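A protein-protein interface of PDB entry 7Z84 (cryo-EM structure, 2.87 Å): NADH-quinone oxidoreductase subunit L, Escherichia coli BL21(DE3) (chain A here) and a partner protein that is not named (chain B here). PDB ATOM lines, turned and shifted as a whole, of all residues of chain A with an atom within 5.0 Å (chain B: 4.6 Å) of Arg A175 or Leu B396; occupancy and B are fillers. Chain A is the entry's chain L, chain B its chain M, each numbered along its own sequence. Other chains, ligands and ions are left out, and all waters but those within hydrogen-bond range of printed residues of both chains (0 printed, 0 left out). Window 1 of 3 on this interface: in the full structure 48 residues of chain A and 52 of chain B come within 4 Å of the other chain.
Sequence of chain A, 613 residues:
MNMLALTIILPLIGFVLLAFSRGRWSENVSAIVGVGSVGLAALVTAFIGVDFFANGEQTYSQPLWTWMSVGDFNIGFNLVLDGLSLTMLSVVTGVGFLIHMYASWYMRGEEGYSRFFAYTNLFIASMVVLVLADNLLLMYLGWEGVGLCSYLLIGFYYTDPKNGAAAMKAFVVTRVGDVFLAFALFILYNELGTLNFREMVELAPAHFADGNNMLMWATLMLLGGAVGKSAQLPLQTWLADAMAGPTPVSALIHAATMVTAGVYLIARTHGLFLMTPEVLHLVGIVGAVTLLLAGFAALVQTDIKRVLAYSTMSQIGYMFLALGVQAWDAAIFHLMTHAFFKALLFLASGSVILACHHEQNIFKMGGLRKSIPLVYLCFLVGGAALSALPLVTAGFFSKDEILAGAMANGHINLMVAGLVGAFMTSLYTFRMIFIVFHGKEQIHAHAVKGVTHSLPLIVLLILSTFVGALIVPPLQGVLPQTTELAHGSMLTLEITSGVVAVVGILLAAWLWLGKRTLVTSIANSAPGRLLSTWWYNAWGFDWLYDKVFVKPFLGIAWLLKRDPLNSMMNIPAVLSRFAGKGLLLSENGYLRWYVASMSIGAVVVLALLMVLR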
ATOM      1  N   GLU A 144     -23.162  25.909   2.096  1.00  0.00           N
ATOM      2  CA  GLU A 144     -22.364  26.728   2.998  1.00  0.00           C
ATOM      3  C   GLU A 144     -23.233  27.564   3.927  1.00  0.00           C
ATOM      4  O   GLU A 144     -22.857  27.780   5.083  1.00  0.00           O
ATOM      5  CB  GLU A 144     -21.430  27.621   2.193  1.00  0.00           C
ATOM      6  CG  GLU A 144     -20.011  27.703   2.727  1.00  0.00           C
ATOM      7  CD  GLU A 144     -19.173  26.500   2.347  1.00  0.00           C
ATOM      8  OE1 GLU A 144     -19.637  25.684   1.525  1.00  0.00           O
ATOM      9  OE2 GLU A 144     -18.047  26.368   2.869  1.00  0.00           O
ATOM     10  N   ALA A 170     -17.522  21.805  14.458  1.00  0.00           N
ATOM     11  CA  ALA A 170     -18.549  21.539  13.456  1.00  0.00           C
ATOM     12  C   ALA A 170     -18.280  22.309  12.170  1.00  0.00           C
ATOM     13  O   ALA A 170     -18.304  21.732  11.074  1.00  0.00           O
ATOM     14  CB  ALA A 170     -19.926  21.890  14.016  1.00  0.00           C
ATOM     15  N   PHE A 171     -17.982  23.609  12.287  1.00  0.00           N
ATOM     16  CA  PHE A 171     -17.766  24.416  11.090  1.00  0.00           C
ATOM     17  C   PHE A 171     -16.494  24.009  10.358  1.00  0.00           C
ATOM     18  O   PHE A 171     -16.471  24.000   9.125  1.00  0.00           O
ATOM     19  CB  PHE A 171     -17.729  25.902  11.441  1.00  0.00           C
ATOM     20  CG  PHE A 171     -17.869  26.806  10.245  1.00  0.00           C
ATOM     21  CD1 PHE A 171     -19.120  27.127   9.745  1.00  0.00           C
ATOM     22  CD2 PHE A 171     -16.751  27.323   9.614  1.00  0.00           C
ATOM     23  CE1 PHE A 171     -19.253  27.954   8.648  1.00  0.00           C
ATOM     24  CE2 PHE A 171     -16.877  28.148   8.514  1.00  0.00           C
ATOM     25  CZ  PHE A 171     -18.131  28.463   8.031  1.00  0.00           C
ATOM     26  N   VAL A 172     -15.439  23.636  11.086  1.00  0.00           N
ATOM     27  CA  VAL A 172     -14.177  23.281  10.438  1.00  0.00           C
ATOM     28  C   VAL A 172     -14.304  21.952   9.695  1.00  0.00           C
ATOM     29  O   VAL A 172     -13.867  21.824   8.542  1.00  0.00           O
ATOM     30  CB  VAL A 172     -13.036  23.259  11.472  1.00  0.00           C
ATOM     31  CG1 VAL A 172     -11.839  22.479  10.956  1.00  0.00           C
ATOM     32  CG2 VAL A 172     -12.621  24.678  11.814  1.00  0.00           C
ATOM     33  N   VAL A 173     -14.923  20.949  10.330  1.00  0.00           N
ATOM     34  CA  VAL A 173     -15.069  19.653   9.668  1.00  0.00           C
ATOM     35  C   VAL A 173     -16.022  19.758   8.479  1.00  0.00           C
ATOM     36  O   VAL A 173     -15.749  19.219   7.391  1.00  0.00           O
ATOM     37  CB  VAL A 173     -15.521  18.587  10.681  1.00  0.00           C
ATOM     38  CG1 VAL A 173     -15.807  17.278   9.981  1.00  0.00           C
ATOM     39  CG2 VAL A 173     -14.455  18.389  11.746  1.00  0.00           C
ATOM     40  N   THR A 174     -17.135  20.485   8.644  1.00  0.00           N
ATOM     41  CA  THR A 174     -18.032  20.684   7.514  1.00  0.00           C
ATOM     42  C   THR A 174     -17.383  21.522   6.420  1.00  0.00           C
ATOM     43  O   THR A 174     -17.673  21.309   5.245  1.00  0.00           O
ATOM     44  CB  THR A 174     -19.344  21.320   7.974  1.00  0.00           C
ATOM     45  OG1 THR A 174     -19.066  22.435   8.828  1.00  0.00           O
ATOM     46  CG2 THR A 174     -20.189  20.307   8.728  1.00  0.00           C
ATOM     47  N   ARG A 175     -16.472  22.435   6.769  1.00  0.00           N
ATOM     48  CA  ARG A 175     -15.775  23.216   5.753  1.00  0.00           C
ATOM     49  C   ARG A 175     -14.780  22.366   4.973  1.00  0.00           C
ATOM     50  O   ARG A 175     -14.584  22.592   3.774  1.00  0.00           O
ATOM     51  CB  ARG A 175     -15.064  24.403   6.403  1.00  0.00           C
ATOM     52  CG  ARG A 175     -14.556  25.433   5.414  1.00  0.00           C
ATOM     53  CD  ARG A 175     -15.623  26.467   5.115  1.00  0.00           C
ATOM     54  NE  ARG A 175     -15.119  27.535   4.261  1.00  0.00           N
ATOM     55  CZ  ARG A 175     -15.848  28.556   3.834  1.00  0.00           C
ATOM     56  NH1 ARG A 175     -17.119  28.689   4.175  1.00  0.00           N
ATOM     57  NH2 ARG A 175     -15.289  29.465   3.041  1.00  0.00           N
ATOM     58  N   VAL A 176     -14.145  21.394   5.631  1.00  0.00           N
ATOM     59  CA  VAL A 176     -13.312  20.431   4.911  1.00  0.00           C
ATOM     60  C   VAL A 176     -14.162  19.625   3.933  1.00  0.00           C
ATOM     61  O   VAL A 176     -13.769  19.393   2.774  1.00  0.00           O
ATOM     62  CB  VAL A 176     -12.565  19.525   5.908  1.00  0.00           C
ATOM     63  CG1 VAL A 176     -11.926  18.350   5.197  1.00  0.00           C
ATOM     64  CG2 VAL A 176     -11.518  20.322   6.665  1.00  0.00           C
ATOM     65  N   GLY A 177     -15.352  19.206   4.378  1.00  0.00           N
ATOM     66  CA  GLY A 177     -16.285  18.552   3.468  1.00  0.00           C
ATOM     67  C   GLY A 177     -16.688  19.431   2.296  1.00  0.00           C
ATOM     68  O   GLY A 177     -16.759  18.969   1.153  1.00  0.00           O
ATOM     69  N   ASP A 178     -16.932  20.717   2.557  1.00  0.00           N
ATOM     70  CA  ASP A 178     -17.290  21.644   1.488  1.00  0.00           C
ATOM     71  C   ASP A 178     -16.128  21.887   0.536  1.00  0.00           C
ATOM     72  O   ASP A 178     -16.348  22.157  -0.644  1.00  0.00           O
ATOM     73  CB  ASP A 178     -17.774  22.974   2.066  1.00  0.00           C
ATOM     74  CG  ASP A 178     -18.927  22.802   3.022  1.00  0.00           C
ATOM     75  OD1 ASP A 178     -19.470  21.683   3.089  1.00  0.00           O
ATOM     76  OD2 ASP A 178     -19.279  23.769   3.727  1.00  0.00           O
ATOM     77  N   VAL A 179     -14.894  21.798   1.025  1.00  0.00           N
ATOM     78  CA  VAL A 179     -13.738  21.935   0.145  1.00  0.00           C
ATOM     79  C   VAL A 179     -13.608  20.720  -0.772  1.00  0.00           C
ATOM     80  O   VAL A 179     -13.286  20.854  -1.962  1.00  0.00           O
ATOM     81  CB  VAL A 179     -12.477  22.199   0.989  1.00  0.00           C
ATOM     82  CG1 VAL A 179     -11.224  21.691   0.315  1.00  0.00           C
ATOM     83  CG2 VAL A 179     -12.358  23.685   1.225  1.00  0.00           C
ATOM     84  N   ALA B 392     -16.734  38.927   9.480  1.00  0.00           N
ATOM     85  CA  ALA B 392     -15.840  37.784   9.636  1.00  0.00           C
ATOM     86  C   ALA B 392     -16.328  36.580   8.839  1.00  0.00           C
ATOM     87  O   ALA B 392     -15.517  35.804   8.318  1.00  0.00           O
ATOM     88  CB  ALA B 392     -15.693  37.431  11.112  1.00  0.00           C
ATOM     89  N   VAL B 393     -17.648  36.397   8.743  1.00  0.00           N
ATOM     90  CA  VAL B 393     -18.188  35.380   7.846  1.00  0.00           C
ATOM     91  C   VAL B 393     -17.955  35.772   6.386  1.00  0.00           C
ATOM     92  O   VAL B 393     -17.775  34.904   5.522  1.00  0.00           O
ATOM     93  CB  VAL B 393     -19.675  35.130   8.179  1.00  0.00           C
ATOM     94  CG1 VAL B 393     -20.303  34.130   7.240  1.00  0.00           C
ATOM     95  CG2 VAL B 393     -19.794  34.568   9.581  1.00  0.00           C
ATOM     96  N   ALA B 394     -17.920  37.073   6.089  1.00  0.00           N
ATOM     97  CA  ALA B 394     -17.649  37.510   4.722  1.00  0.00           C
ATOM     98  C   ALA B 394     -16.221  37.176   4.294  1.00  0.00           C
ATOM     99  O   ALA B 394     -16.004  36.674   3.186  1.00  0.00           O
ATOM    100  CB  ALA B 394     -17.923  39.007   4.583  1.00  0.00           C
ATOM    101  N   THR B 395     -15.230  37.430   5.157  1.00  0.00           N
ATOM    102  CA  THR B 395     -13.848  37.183   4.744  1.00  0.00           C
ATOM    103  C   THR B 395     -13.443  35.711   4.746  1.00  0.00           C
ATOM    104  O   THR B 395     -12.337  35.403   4.291  1.00  0.00           O
ATOM    105  CB  THR B 395     -12.838  37.961   5.603  1.00  0.00           C
ATOM    106  OG1 THR B 395     -12.482  37.197   6.764  1.00  0.00           O
ATOM    107  CG2 THR B 395     -13.336  39.341   5.975  1.00  0.00           C
ATOM    108  N   LEU B 396     -14.276  34.795   5.234  1.00  0.00           N
ATOM    109  CA  LEU B 396     -13.938  33.383   5.111  1.00  0.00           C
ATOM    110  C   LEU B 396     -14.461  32.767   3.820  1.00  0.00           C
ATOM    111  O   LEU B 396     -14.270  31.567   3.601  1.00  0.00           O
ATOM    112  CB  LEU B 396     -14.447  32.576   6.317  1.00  0.00           C
ATOM    113  CG  LEU B 396     -15.903  32.577   6.789  1.00  0.00           C
ATOM    114  CD1 LEU B 396     -16.695  31.453   6.148  1.00  0.00           C
ATOM    115  CD2 LEU B 396     -15.960  32.446   8.298  1.00  0.00           C
ATOM    116  N   GLY B 397     -15.109  33.554   2.965  1.00  0.00           N
ATOM    117  CA  GLY B 397     -15.571  33.064   1.682  1.00  0.00           C
ATOM    118  C   GLY B 397     -16.959  32.464   1.721  1.00  0.00           C
ATOM    119  O   GLY B 397     -17.195  31.392   1.159  1.00  0.00           O
ATOM    120  N   MET B 398     -17.885  33.144   2.381  1.00  0.00           N
ATOM    121  CA  MET B 398     -19.243  32.628   2.491  1.00  0.00           C
ATOM    122  C   MET B 398     -20.086  33.105   1.314  1.00  0.00           C
ATOM    123  O   MET B 398     -20.046  34.292   0.972  1.00  0.00           O
ATOM    124  CB  MET B 398     -19.880  33.063   3.802  1.00  0.00           C
ATOM    125  CG  MET B 398     -21.370  32.772   3.909  1.00  0.00           C
ATOM    126  SD  MET B 398     -21.778  31.127   4.538  1.00  0.00           S
ATOM    127  CE  MET B 398     -20.304  30.700   5.462  1.00  0.00           C
ATOM    128  N   LEU B 429      -8.509  28.110   2.079  1.00  0.00           N
ATOM    129  CA  LEU B 429      -9.824  28.647   2.443  1.00  0.00           C
ATOM    130  C   LEU B 429     -10.332  28.036   3.746  1.00  0.00           C
ATOM    131  O   LEU B 429     -10.979  28.719   4.556  1.00  0.00           O
ATOM    132  CB  LEU B 429     -10.842  28.408   1.329  1.00  0.00           C
ATOM    133  CG  LEU B 429     -10.925  29.397   0.170  1.00  0.00           C
ATOM    134  CD1 LEU B 429     -11.789  28.829  -0.938  1.00  0.00           C
ATOM    135  CD2 LEU B 429     -11.466  30.737   0.641  1.00  0.00           C
ATOM    136  N   VAL B 430     -10.070  26.739   3.947  1.00  0.00           N
ATOM    137  CA  VAL B 430     -10.359  26.113   5.245  1.00  0.00           C
ATOM    138  C   VAL B 430      -9.608  26.832   6.364  1.00  0.00           C
ATOM    139  O   VAL B 430     -10.177  27.144   7.423  1.00  0.00           O
ATOM    140  CB  VAL B 430     -10.020  24.608   5.210  1.00  0.00           C
ATOM    141  CG1 VAL B 430      -9.759  24.067   6.609  1.00  0.00           C
ATOM    142  CG2 VAL B 430     -11.152  23.837   4.605  1.00  0.00           C
ATOM    143  N   ALA B 432      -8.634  29.899   6.324  1.00  0.00           N
ATOM    144  CA  ALA B 432      -9.256  31.212   6.466  1.00  0.00           C
ATOM    145  C   ALA B 432     -10.486  31.152   7.359  1.00  0.00           C
ATOM    146  O   ALA B 432     -10.688  32.024   8.219  1.00  0.00           O
ATOM    147  CB  ALA B 432      -9.618  31.771   5.091  1.00  0.00           C
ATOM    148  N   SER B 433     -11.318  30.125   7.167  1.00  0.00           N
ATOM    149  CA  SER B 433     -12.457  29.919   8.059  1.00  0.00           C
ATOM    150  C   SER B 433     -11.993  29.700   9.495  1.00  0.00           C
ATOM    151  O   SER B 433     -12.615  30.207  10.440  1.00  0.00           O
ATOM    152  CB  SER B 433     -13.296  28.737   7.579  1.00  0.00           C
ATOM    153  OG  SER B 433     -12.800  27.518   8.100  1.00  0.00           O
ATOM    154  N   SER B 436     -10.974  33.063  11.011  1.00  0.00           N
ATOM    155  CA  SER B 436     -12.140  33.918  11.217  1.00  0.00           C
ATOM    156  C   SER B 436     -12.927  33.493  12.453  1.00  0.00           C
ATOM    157  O   SER B 436     -13.328  34.342  13.264  1.00  0.00           O
ATOM    158  CB  SER B 436     -13.031  33.902   9.978  1.00  0.00           C
ATOM    159  OG  SER B 436     -12.350  34.433   8.856  1.00  0.00           O
ATOM    160  N   LEU B 437     -13.131  32.181  12.627  1.00  0.00           N
ATOM    161  CA  LEU B 437     -13.811  31.700  13.827  1.00  0.00           C
ATOM    162  C   LEU B 437     -12.994  31.978  15.083  1.00  0.00           C
ATOM    163  O   LEU B 437     -13.561  32.303  16.136  1.00  0.00           O
ATOM    164  CB  LEU B 437     -14.107  30.207  13.719  1.00  0.00           C
ATOM    165  CG  LEU B 437     -14.973  29.732  12.557  1.00  0.00           C
ATOM    166  CD1 LEU B 437     -15.303  28.269  12.758  1.00  0.00           C
ATOM    167  CD2 LEU B 437     -16.224  30.578  12.401  1.00  0.00           C
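The guanidinium group (NH2) of Arg A175 lies within hydrogen-bond range of the backbone carbonyl oxygen (O) of Gly B397 (3.3 Å). The backbone carbonyl oxygen (O) of Glu A144 lies close to the side-chain sulfur (SD) of Met B398 (3.6 Å). The backbone carbonyl oxygen of Leu B396 sits at hydrogen-bond distance from the guanidinium group of Arg A175.
Of the printed residues of chain B, Arg A175 touches Leu B396, Gly B397, Met B398, Val B430 and Ser B433. Of the printed residues of chain B, Val A176 touches Val B430. Printed residues of chain B within 4 Å of Val A179: Val B430. Of chain A, only Phe A171 (3.8 Å) and Arg A175 (2.4 Å) come within 4 Å of Leu B396. Of the printed residues of chain A, Gly B397 touches Arg A175. Printed residues of chain A within 4 Å of Leu B437: Phe A171 (3.6 Å). The nearest printed residue of chain B that does not touch Glu A144 is Gly B397 (4.9 Å).
Of the 11 printed residues of chain A, 5 touch a printed residue of chain B. Printed residues of chain A that touch a printed residue of chain B: Glu A144, Phe A171, Arg A175, Val A176 and Val A179. Hydrophobic or aromatic side chains of chain A within 4 Å of the printed part of chain B: Phe A171 and Val A179. Printed residues of chain B that touch a printed residue of chain A: Leu B396, Gly B397, Met B398, Val B430, Ser B433 and Leu B437. Among the printed residues, no Asp or Glu carboxylate lies within 4 Å of a Lys or Arg side-chain nitrogen of the other chain.
Among the printed residues, pairs that only touch across the chains: Phe A171 with Leu B396 (3.8 Å), Phe A171 with Ser B433 (3.7 Å), Phe A171 with Leu B437 (3.6 Å), Arg A175 with Met B398 (3.98 Å), Arg A175 with Val B430 (3.7 Å), Arg A175 with Ser B433 (3.8 Å), Val A176 with Val B430 (3.997 Å) and Val A179 with Val B430 (3.6 Å).
The side-chain hydroxyl (OG1) of Thr A174 is in hydrogen-bond range of the backbone carbonyl oxygen (O) of Phe A171, 3.0 Å away. OE2 of Glu A144 lies within salt-bridge range of NH1 of Arg A175 (2.8 Å). The backbone carbonyl oxygen of Val B430 is in hydrogen-bond range of the side-chain hydroxyl of Ser B433 (2.7 Å).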
